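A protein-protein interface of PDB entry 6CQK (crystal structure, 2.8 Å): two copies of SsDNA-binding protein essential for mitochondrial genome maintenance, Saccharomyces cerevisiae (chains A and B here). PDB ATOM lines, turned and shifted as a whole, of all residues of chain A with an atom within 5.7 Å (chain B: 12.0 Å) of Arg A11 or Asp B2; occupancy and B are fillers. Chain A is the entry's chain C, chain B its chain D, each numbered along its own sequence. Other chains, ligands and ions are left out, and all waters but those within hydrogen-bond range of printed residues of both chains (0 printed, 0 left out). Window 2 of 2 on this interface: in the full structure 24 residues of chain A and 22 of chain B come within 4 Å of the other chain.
Arg A11 touches just one residue of chain B: Asp B2.
Val A9 touches just these residues of chain B: Asp B2 (3.2 Å) and Phe B3 (2.9 Å).
Of chain B, only Asp B2 (3.6 Å) comes within 4 Å of Gly A10.
No residue of chain B comes within 4 Å of Gly A13.
No residue of chain B comes within 4 Å of Ile A32.
Ala A33 touches just one residue of chain B: Asp B2 (3.5 Å).
Ser A34 touches two residues of chain B.
Of chain B, only Asp B2 comes within 4 Å of Leu A67.
Of the printed residues of chain A, Phe B3 touches Val A9 (2.9 Å) and Ser A34 (3.3 Å).
The nearest printed residue of chain A that does not touch Asp B2 is Val A68 (6.4 Å).
The nearest printed residue of chain A that does not touch Phe B3 is Gly A10 (5.0 Å).
Among the printed residues, merely in contact across the chains: Val A9 with Asp B2 (3.2 Å), Gly A10 with Asp B2 (3.6 Å), Ser A34 with Asp B2 (3.4 Å), Pro A36 with Asp B2 (3.6 Å) and Leu A67 with Asp B2 (3.6 Å).
N of Val A9 lies within hydrogen-bond range of O of Phe B3.
The guanidinium group of Arg A11 lies within salt-bridge range of the side-chain carboxylate of Asp B2 (2.7 Å).
The backbone NH (N) of Gln A35 sits at hydrogen-bond distance from the side-chain carboxylate (OD2) of Asp B2.
The side-chain hydroxyl (OG) of Ser A34 lies within hydrogen-bond range of the backbone carbonyl oxygen (O) of Phe B3.
The backbone carbonyl oxygen (O) of Ala A33 sits close to the side-chain carboxylate (OD2) of Asp B2 (3.5 Å).
O of Arg A11 sits at hydrogen-bond distance from N of Ala A33.
The backbone carbonyl oxygen of Gly A10 sits at hydrogen-bond distance from the backbone NH of Val A68 (2.9 Å).
The backbone carbonyl oxygen of Val A9 is in hydrogen-bond range of the side-chain hydroxyl of Ser A34 (3.3 Å).
No position is printed for both chains.
Of the 10 pairs that touch across the chains among the printed residues, none has its exchanged pair printed and touching as well.
Printed residues of chain A that touch a printed residue of chain B: Val A9, Gly A10, Arg A11, Ala A33, Ser A34, Gln A35, Pro A36 and Leu A67.
Hydrophobic or aromatic side chains of chain A within 4 Å of the printed part of chain B: Val A9, Pro A36 and Leu A67.
Hydrophobic or aromatic side chains of chain B that line the printed part of chain A: Phe B3.
Along chain B the printed residues that touch a printed residue of chain A span positions 2 to 3.
Among the printed residues, 10 pairs touch across the chains.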
ATOM      1  N   VAL A   9      14.167 -10.936 -23.452  1.00  0.00           N
ATOM      2  CA  VAL A   9      13.865 -11.282 -22.097  1.00  0.00           C
ATOM      3  C   VAL A   9      13.220 -12.639 -22.100  1.00  0.00           C
ATOM      4  O   VAL A   9      12.180 -12.869 -22.763  1.00  0.00           O
ATOM      5  CB  VAL A   9      12.937 -10.266 -21.411  1.00  0.00           C
ATOM      6  CG1 VAL A   9      12.481 -10.767 -20.038  1.00  0.00           C
ATOM      7  CG2 VAL A   9      13.674  -8.947 -21.239  1.00  0.00           C
ATOM      8  N   GLY A  10      13.774 -13.488 -21.251  1.00  0.00           N
ATOM      9  CA  GLY A  10      13.306 -14.849 -21.130  1.00  0.00           C
ATOM     10  C   GLY A  10      13.989 -15.626 -20.039  1.00  0.00           C
ATOM     11  O   GLY A  10      14.795 -15.072 -19.283  1.00  0.00           O
ATOM     12  N   ARG A  11      13.730 -16.918 -20.009  1.00  0.00           N
ATOM     13  CA  ARG A  11      14.276 -17.753 -18.981  1.00  0.00           C
ATOM     14  C   ARG A  11      15.292 -18.676 -19.548  1.00  0.00           C
ATOM     15  O   ARG A  11      15.177 -19.170 -20.661  1.00  0.00           O
ATOM     16  CB  ARG A  11      13.182 -18.527 -18.283  1.00  0.00           C
ATOM     17  CG  ARG A  11      12.616 -17.829 -17.043  1.00  0.00           C
ATOM     18  CD  ARG A  11      11.206 -18.328 -16.648  1.00  0.00           C
ATOM     19  NE  ARG A  11      10.307 -17.209 -16.335  1.00  0.00           N
ATOM     20  CZ  ARG A  11       9.541 -16.517 -17.205  1.00  0.00           C
ATOM     21  NH1 ARG A  11       9.508 -16.765 -18.522  1.00  0.00           N
ATOM     22  NH2 ARG A  11       8.779 -15.528 -16.723  1.00  0.00           N
ATOM     23  N   ILE A  12      16.329 -18.906 -18.775  1.00  0.00           N
ATOM     24  CA  ILE A  12      17.383 -19.802 -19.218  1.00  0.00           C
ATOM     25  C   ILE A  12      16.887 -21.226 -19.179  1.00  0.00           C
ATOM     26  O   ILE A  12      16.547 -21.727 -18.110  1.00  0.00           O
ATOM     27  CB  ILE A  12      18.661 -19.607 -18.399  1.00  0.00           C
ATOM     28  CG1 ILE A  12      19.227 -18.256 -18.838  1.00  0.00           C
ATOM     29  CG2 ILE A  12      19.617 -20.764 -18.635  1.00  0.00           C
ATOM     30  CD1 ILE A  12      20.568 -17.896 -18.297  1.00  0.00           C
ATOM     31  N   GLY A  13      16.848 -21.853 -20.354  1.00  0.00           N
ATOM     32  CA  GLY A  13      16.266 -23.156 -20.488  1.00  0.00           C
ATOM     33  C   GLY A  13      17.252 -24.245 -20.748  1.00  0.00           C
ATOM     34  O   GLY A  13      16.879 -25.288 -21.280  1.00  0.00           O
ATOM     35  N   SER A  31      20.519 -21.929 -24.145  1.00  0.00           N
ATOM     36  CA  SER A  31      19.302 -21.490 -24.799  1.00  0.00           C
ATOM     37  C   SER A  31      18.411 -20.726 -23.816  1.00  0.00           C
ATOM     38  O   SER A  31      18.406 -21.002 -22.619  1.00  0.00           O
ATOM     39  CB  SER A  31      18.585 -22.687 -25.420  1.00  0.00           C
ATOM     40  OG  SER A  31      18.428 -23.703 -24.464  1.00  0.00           O
ATOM     41  N   ILE A  32      17.681 -19.752 -24.351  1.00  0.00           N
ATOM     42  CA  ILE A  32      16.713 -18.972 -23.610  1.00  0.00           C
ATOM     43  C   ILE A  32      15.359 -19.363 -24.143  1.00  0.00           C
ATOM     44  O   ILE A  32      15.113 -19.254 -25.357  1.00  0.00           O
ATOM     45  CB  ILE A  32      16.927 -17.438 -23.839  1.00  0.00           C
ATOM     46  CG1 ILE A  32      18.293 -17.003 -23.313  1.00  0.00           C
ATOM     47  CG2 ILE A  32      15.862 -16.572 -23.149  1.00  0.00           C
ATOM     48  CD1 ILE A  32      18.684 -15.575 -23.631  1.00  0.00           C
ATOM     49  N   ALA A  33      14.430 -19.697 -23.249  1.00  0.00           N
ATOM     50  CA  ALA A  33      13.002 -19.819 -23.626  1.00  0.00           C
ATOM     51  C   ALA A  33      12.282 -18.512 -23.352  1.00  0.00           C
ATOM     52  O   ALA A  33      12.318 -18.047 -22.217  1.00  0.00           O
ATOM     53  CB  ALA A  33      12.369 -20.910 -22.852  1.00  0.00           C
ATOM     54  N   SER A  34      11.760 -17.862 -24.398  1.00  0.00           N
ATOM     55  CA  SER A  34      11.096 -16.570 -24.253  1.00  0.00           C
ATOM     56  C   SER A  34       9.715 -16.887 -24.671  1.00  0.00           C
ATOM     57  O   SER A  34       9.464 -17.262 -25.798  1.00  0.00           O
ATOM     58  CB  SER A  34      11.694 -15.455 -25.108  1.00  0.00           C
ATOM     59  OG  SER A  34      10.780 -14.354 -25.318  1.00  0.00           O
ATOM     60  N   GLN A  35       8.823 -16.735 -23.694  1.00  0.00           N
ATOM     61  CA  GLN A  35       7.444 -17.093 -23.829  1.00  0.00           C
ATOM     62  C   GLN A  35       6.567 -15.932 -23.429  1.00  0.00           C
ATOM     63  O   GLN A  35       6.272 -15.751 -22.211  1.00  0.00           O
ATOM     64  CB  GLN A  35       7.125 -18.278 -22.970  1.00  0.00           C
ATOM     65  CG  GLN A  35       5.710 -18.728 -23.235  1.00  0.00           C
ATOM     66  CD  GLN A  35       5.330 -19.906 -22.399  1.00  0.00           C
ATOM     67  OE1 GLN A  35       5.943 -20.194 -21.377  1.00  0.00           O
ATOM     68  NE2 GLN A  35       4.299 -20.569 -22.809  1.00  0.00           N
ATOM     69  N   PRO A  36       6.152 -15.138 -24.430  1.00  0.00           N
ATOM     70  CA  PRO A  36       5.354 -13.992 -24.116  1.00  0.00           C
ATOM     71  C   PRO A  36       4.047 -14.333 -23.384  1.00  0.00           C
ATOM     72  O   PRO A  36       3.605 -13.493 -22.622  1.00  0.00           O
ATOM     73  CB  PRO A  36       5.118 -13.375 -25.484  1.00  0.00           C
ATOM     74  CG  PRO A  36       6.304 -13.751 -26.253  1.00  0.00           C
ATOM     75  CD  PRO A  36       6.647 -15.112 -25.810  1.00  0.00           C
ATOM     76  N   GLY A  65      16.768 -21.510 -15.273  1.00  0.00           N
ATOM     77  CA  GLY A  65      15.452 -20.946 -14.957  1.00  0.00           C
ATOM     78  C   GLY A  65      15.490 -19.469 -14.646  1.00  0.00           C
ATOM     79  O   GLY A  65      14.452 -18.829 -14.426  1.00  0.00           O
ATOM     80  N   ALA A  66      16.684 -18.903 -14.640  1.00  0.00           N
ATOM     81  CA  ALA A  66      16.805 -17.468 -14.432  1.00  0.00           C
ATOM     82  C   ALA A  66      16.101 -16.632 -15.513  1.00  0.00           C
ATOM     83  O   ALA A  66      16.353 -16.813 -16.708  1.00  0.00           O
ATOM     84  CB  ALA A  66      18.274 -17.087 -14.400  1.00  0.00           C
ATOM     85  N   LEU A  67      15.285 -15.684 -15.077  1.00  0.00           N
ATOM     86  CA  LEU A  67      14.861 -14.572 -15.931  1.00  0.00           C
ATOM     87  C   LEU A  67      16.025 -13.616 -16.205  1.00  0.00           C
ATOM     88  O   LEU A  67      16.620 -13.087 -15.261  1.00  0.00           O
ATOM     89  CB  LEU A  67      13.745 -13.772 -15.287  1.00  0.00           C
ATOM     90  CG  LEU A  67      13.098 -12.752 -16.232  1.00  0.00           C
ATOM     91  CD1 LEU A  67      12.407 -13.434 -17.394  1.00  0.00           C
ATOM     92  CD2 LEU A  67      12.090 -11.902 -15.478  1.00  0.00           C
ATOM     93  N   VAL A  68      16.352 -13.448 -17.492  1.00  0.00           N
ATOM     94  CA  VAL A  68      17.479 -12.662 -17.957  1.00  0.00           C
ATOM     95  C   VAL A  68      17.095 -11.689 -19.054  1.00  0.00           C
ATOM     96  O   VAL A  68      16.062 -11.847 -19.683  1.00  0.00           O
ATOM     97  CB  VAL A  68      18.594 -13.509 -18.541  1.00  0.00           C
ATOM     98  CG1 VAL A  68      19.188 -14.368 -17.475  1.00  0.00           C
ATOM     99  CG2 VAL A  68      18.139 -14.379 -19.711  1.00  0.00           C
ATOM    100  N   MET B   1       6.937  -9.582 -18.763  1.00  0.00           N
ATOM    101  CA  MET B   1       6.730 -10.697 -19.709  1.00  0.00           C
ATOM    102  C   MET B   1       7.874 -10.853 -20.619  1.00  0.00           C
ATOM    103  O   MET B   1       8.520  -9.905 -20.969  1.00  0.00           O
ATOM    104  CB  MET B   1       5.491 -10.497 -20.603  1.00  0.00           C
ATOM    105  CG  MET B   1       5.621  -9.634 -21.860  1.00  0.00           C
ATOM    106  SD  MET B   1       4.037  -9.446 -22.727  1.00  0.00           S
ATOM    107  CE  MET B   1       3.965  -7.633 -22.975  1.00  0.00           C
ATOM    108  N   ASP B   2       8.061 -12.062 -21.092  1.00  0.00           N
ATOM    109  CA  ASP B   2       9.136 -12.330 -22.060  1.00  0.00           C
ATOM    110  C   ASP B   2       8.978 -11.572 -23.368  1.00  0.00           C
ATOM    111  O   ASP B   2       7.887 -11.385 -23.846  1.00  0.00           O
ATOM    112  CB  ASP B   2       9.197 -13.834 -22.335  1.00  0.00           C
ATOM    113  CG  ASP B   2       9.758 -14.664 -21.079  1.00  0.00           C
ATOM    114  OD1 ASP B   2      10.004 -14.018 -20.016  1.00  0.00           O
ATOM    115  OD2 ASP B   2       9.787 -15.948 -21.052  1.00  0.00           O
ATOM    116  N   PHE B   3      10.096 -11.140 -23.946  1.00  0.00           N
ATOM    117  CA  PHE B   3      10.073 -10.607 -25.319  1.00  0.00           C
ATOM    118  C   PHE B   3      11.327 -10.920 -26.099  1.00  0.00           C
ATOM    119  O   PHE B   3      12.291 -11.426 -25.550  1.00  0.00           O
ATOM    120  CB  PHE B   3       9.772  -9.117 -25.357  1.00  0.00           C
ATOM    121  CG  PHE B   3      10.920  -8.251 -24.940  1.00  0.00           C
ATOM    122  CD1 PHE B   3      11.844  -7.809 -25.869  1.00  0.00           C
ATOM    123  CD2 PHE B   3      11.059  -7.818 -23.615  1.00  0.00           C
ATOM    124  CE1 PHE B   3      12.898  -6.977 -25.483  1.00  0.00           C
ATOM    125  CE2 PHE B   3      12.097  -6.976 -23.223  1.00  0.00           C
ATOM    126  CZ  PHE B   3      13.031  -6.565 -24.156  1.00  0.00           C
ATOM    127  N   SER B   4      11.284 -10.644 -27.393  1.00  0.00           N
ATOM    128  CA  SER B   4      12.444 -10.823 -28.222  1.00  0.00           C
ATOM    129  C   SER B   4      12.356  -9.932 -29.444  1.00  0.00           C
ATOM    130  O   SER B   4      11.691 -10.274 -30.376  1.00  0.00           O
ATOM    131  CB  SER B   4      12.624 -12.294 -28.623  1.00  0.00           C
ATOM    132  OG  SER B   4      11.554 -12.779 -29.348  1.00  0.00           O
ATOM    133  N   LYS B   5      13.044  -8.805 -29.430  1.00  0.00           N
ATOM    134  CA  LYS B   5      13.018  -7.884 -30.560  1.00  0.00           C
ATOM    135  C   LYS B   5      14.363  -7.843 -31.221  1.00  0.00           C
ATOM    136  O   LYS B   5      15.353  -8.081 -30.571  1.00  0.00           O
ATOM    137  CB  LYS B   5      12.579  -6.475 -30.184  1.00  0.00           C
ATOM    138  CG  LYS B   5      13.413  -5.825 -29.119  1.00  0.00           C
ATOM    139  CD  LYS B   5      12.890  -4.469 -28.704  1.00  0.00           C
ATOM    140  CE  LYS B   5      13.527  -3.420 -29.635  1.00  0.00           C
ATOM    141  NZ  LYS B   5      12.828  -2.098 -29.664  1.00  0.00           N
ATOM    142  N   MET B   6      14.358  -7.538 -32.522  1.00  0.00           N
ATOM    143  CA  MET B   6      15.558  -7.351 -33.341  1.00  0.00           C
ATOM    144  C   MET B   6      15.626  -5.933 -33.906  1.00  0.00           C
ATOM    145  O   MET B   6      14.617  -5.373 -34.300  1.00  0.00           O
ATOM    146  CB  MET B   6      15.512  -8.268 -34.534  1.00  0.00           C
ATOM    147  CG  MET B   6      16.776  -8.234 -35.349  1.00  0.00           C
ATOM    148  SD  MET B   6      17.394  -9.897 -35.666  1.00  0.00           S
ATOM    149  CE  MET B   6      18.248  -9.761 -37.167  1.00  0.00           C
ATOM    150  N   ALA B  72      11.985  -5.039 -35.251  1.00  0.00           N
ATOM    151  CA  ALA B  72      10.994  -6.052 -35.501  1.00  0.00           C
ATOM    152  C   ALA B  72      10.849  -6.992 -34.342  1.00  0.00           C
ATOM    153  O   ALA B  72      11.798  -7.342 -33.647  1.00  0.00           O
ATOM    154  CB  ALA B  72      11.371  -6.803 -36.739  1.00  0.00           C
ATOM    155  N   ASP B  73       9.627  -7.382 -34.087  1.00  0.00           N
ATOM    156  CA  ASP B  73       9.407  -8.376 -33.096  1.00  0.00           C
ATOM    157  C   ASP B  73       9.805  -9.747 -33.676  1.00  0.00           C
ATOM    158  O   ASP B  73       9.444 -10.091 -34.816  1.00  0.00           O
ATOM    159  CB  ASP B  73       7.989  -8.257 -32.558  1.00  0.00           C
ATOM    160  CG  ASP B  73       7.714  -9.288 -31.472  1.00  0.00           C
ATOM    161  OD1 ASP B  73       7.818 -10.575 -31.603  1.00  0.00           O
ATOM    162  OD2 ASP B  73       7.468  -8.761 -30.399  1.00  0.00           O
ATOM    163  N   ALA B  74      10.561 -10.525 -32.884  1.00  0.00           N
ATOM    164  CA  ALA B  74      11.075 -11.814 -33.338  1.00  0.00           C
ATOM    165  C   ALA B  74      10.401 -12.969 -32.690  1.00  0.00           C
ATOM    166  O   ALA B  74      10.132 -12.937 -31.482  1.00  0.00           O
ATOM    167  CB  ALA B  74      12.546 -11.903 -33.061  1.00  0.00           C
ATOM    168  N   ALA B  75      10.135 -14.004 -33.478  1.00  0.00           N
ATOM    169  CA  ALA B  75       9.724 -15.311 -32.912  1.00  0.00           C
ATOM    170  C   ALA B  75      10.408 -16.444 -33.637  1.00  0.00           C
ATOM    171  O   ALA B  75      10.770 -16.260 -34.789  1.00  0.00           O
ATOM    172  CB  ALA B  75       8.208 -15.465 -33.020  1.00  0.00           C
ATOM    173  N   ASN B  76      10.432 -17.611 -33.000  1.00  0.00           N
ATOM    174  CA  ASN B  76      10.887 -18.843 -33.562  1.00  0.00           C
ATOM    175  C   ASN B  76       9.677 -19.845 -33.556  1.00  0.00           C
ATOM    176  O   ASN B  76       9.772 -21.108 -33.616  1.00  0.00           O
ATOM    177  CB  ASN B  76      12.034 -19.329 -32.715  1.00  0.00           C
ATOM    178  CG  ASN B  76      13.425 -18.839 -33.240  1.00  0.00           C
ATOM    179  OD1 ASN B  76      13.687 -18.641 -34.448  1.00  0.00           O
ATOM    180  ND2 ASN B  76      14.362 -18.757 -32.322  1.00  0.00           N
ATOM    181  N   LYS B  95       7.985  -3.446 -36.385  1.00  0.00           N
ATOM    182  CA  LYS B  95       7.371  -2.494 -35.443  1.00  0.00           C
ATOM    183  C   LYS B  95       7.575  -1.083 -35.823  1.00  0.00           C
ATOM    184  O   LYS B  95       6.863  -0.221 -35.365  1.00  0.00           O
ATOM    185  CB  LYS B  95       8.017  -2.607 -34.035  1.00  0.00           C
ATOM    186  CG  LYS B  95       7.073  -3.142 -33.027  1.00  0.00           C
ATOM    187  CD  LYS B  95       6.003  -2.133 -32.583  1.00  0.00           C
ATOM    188  CE  LYS B  95       5.101  -2.729 -31.510  1.00  0.00           C
ATOM    189  NZ  LYS B  95       3.742  -2.108 -31.404  1.00  0.00           N
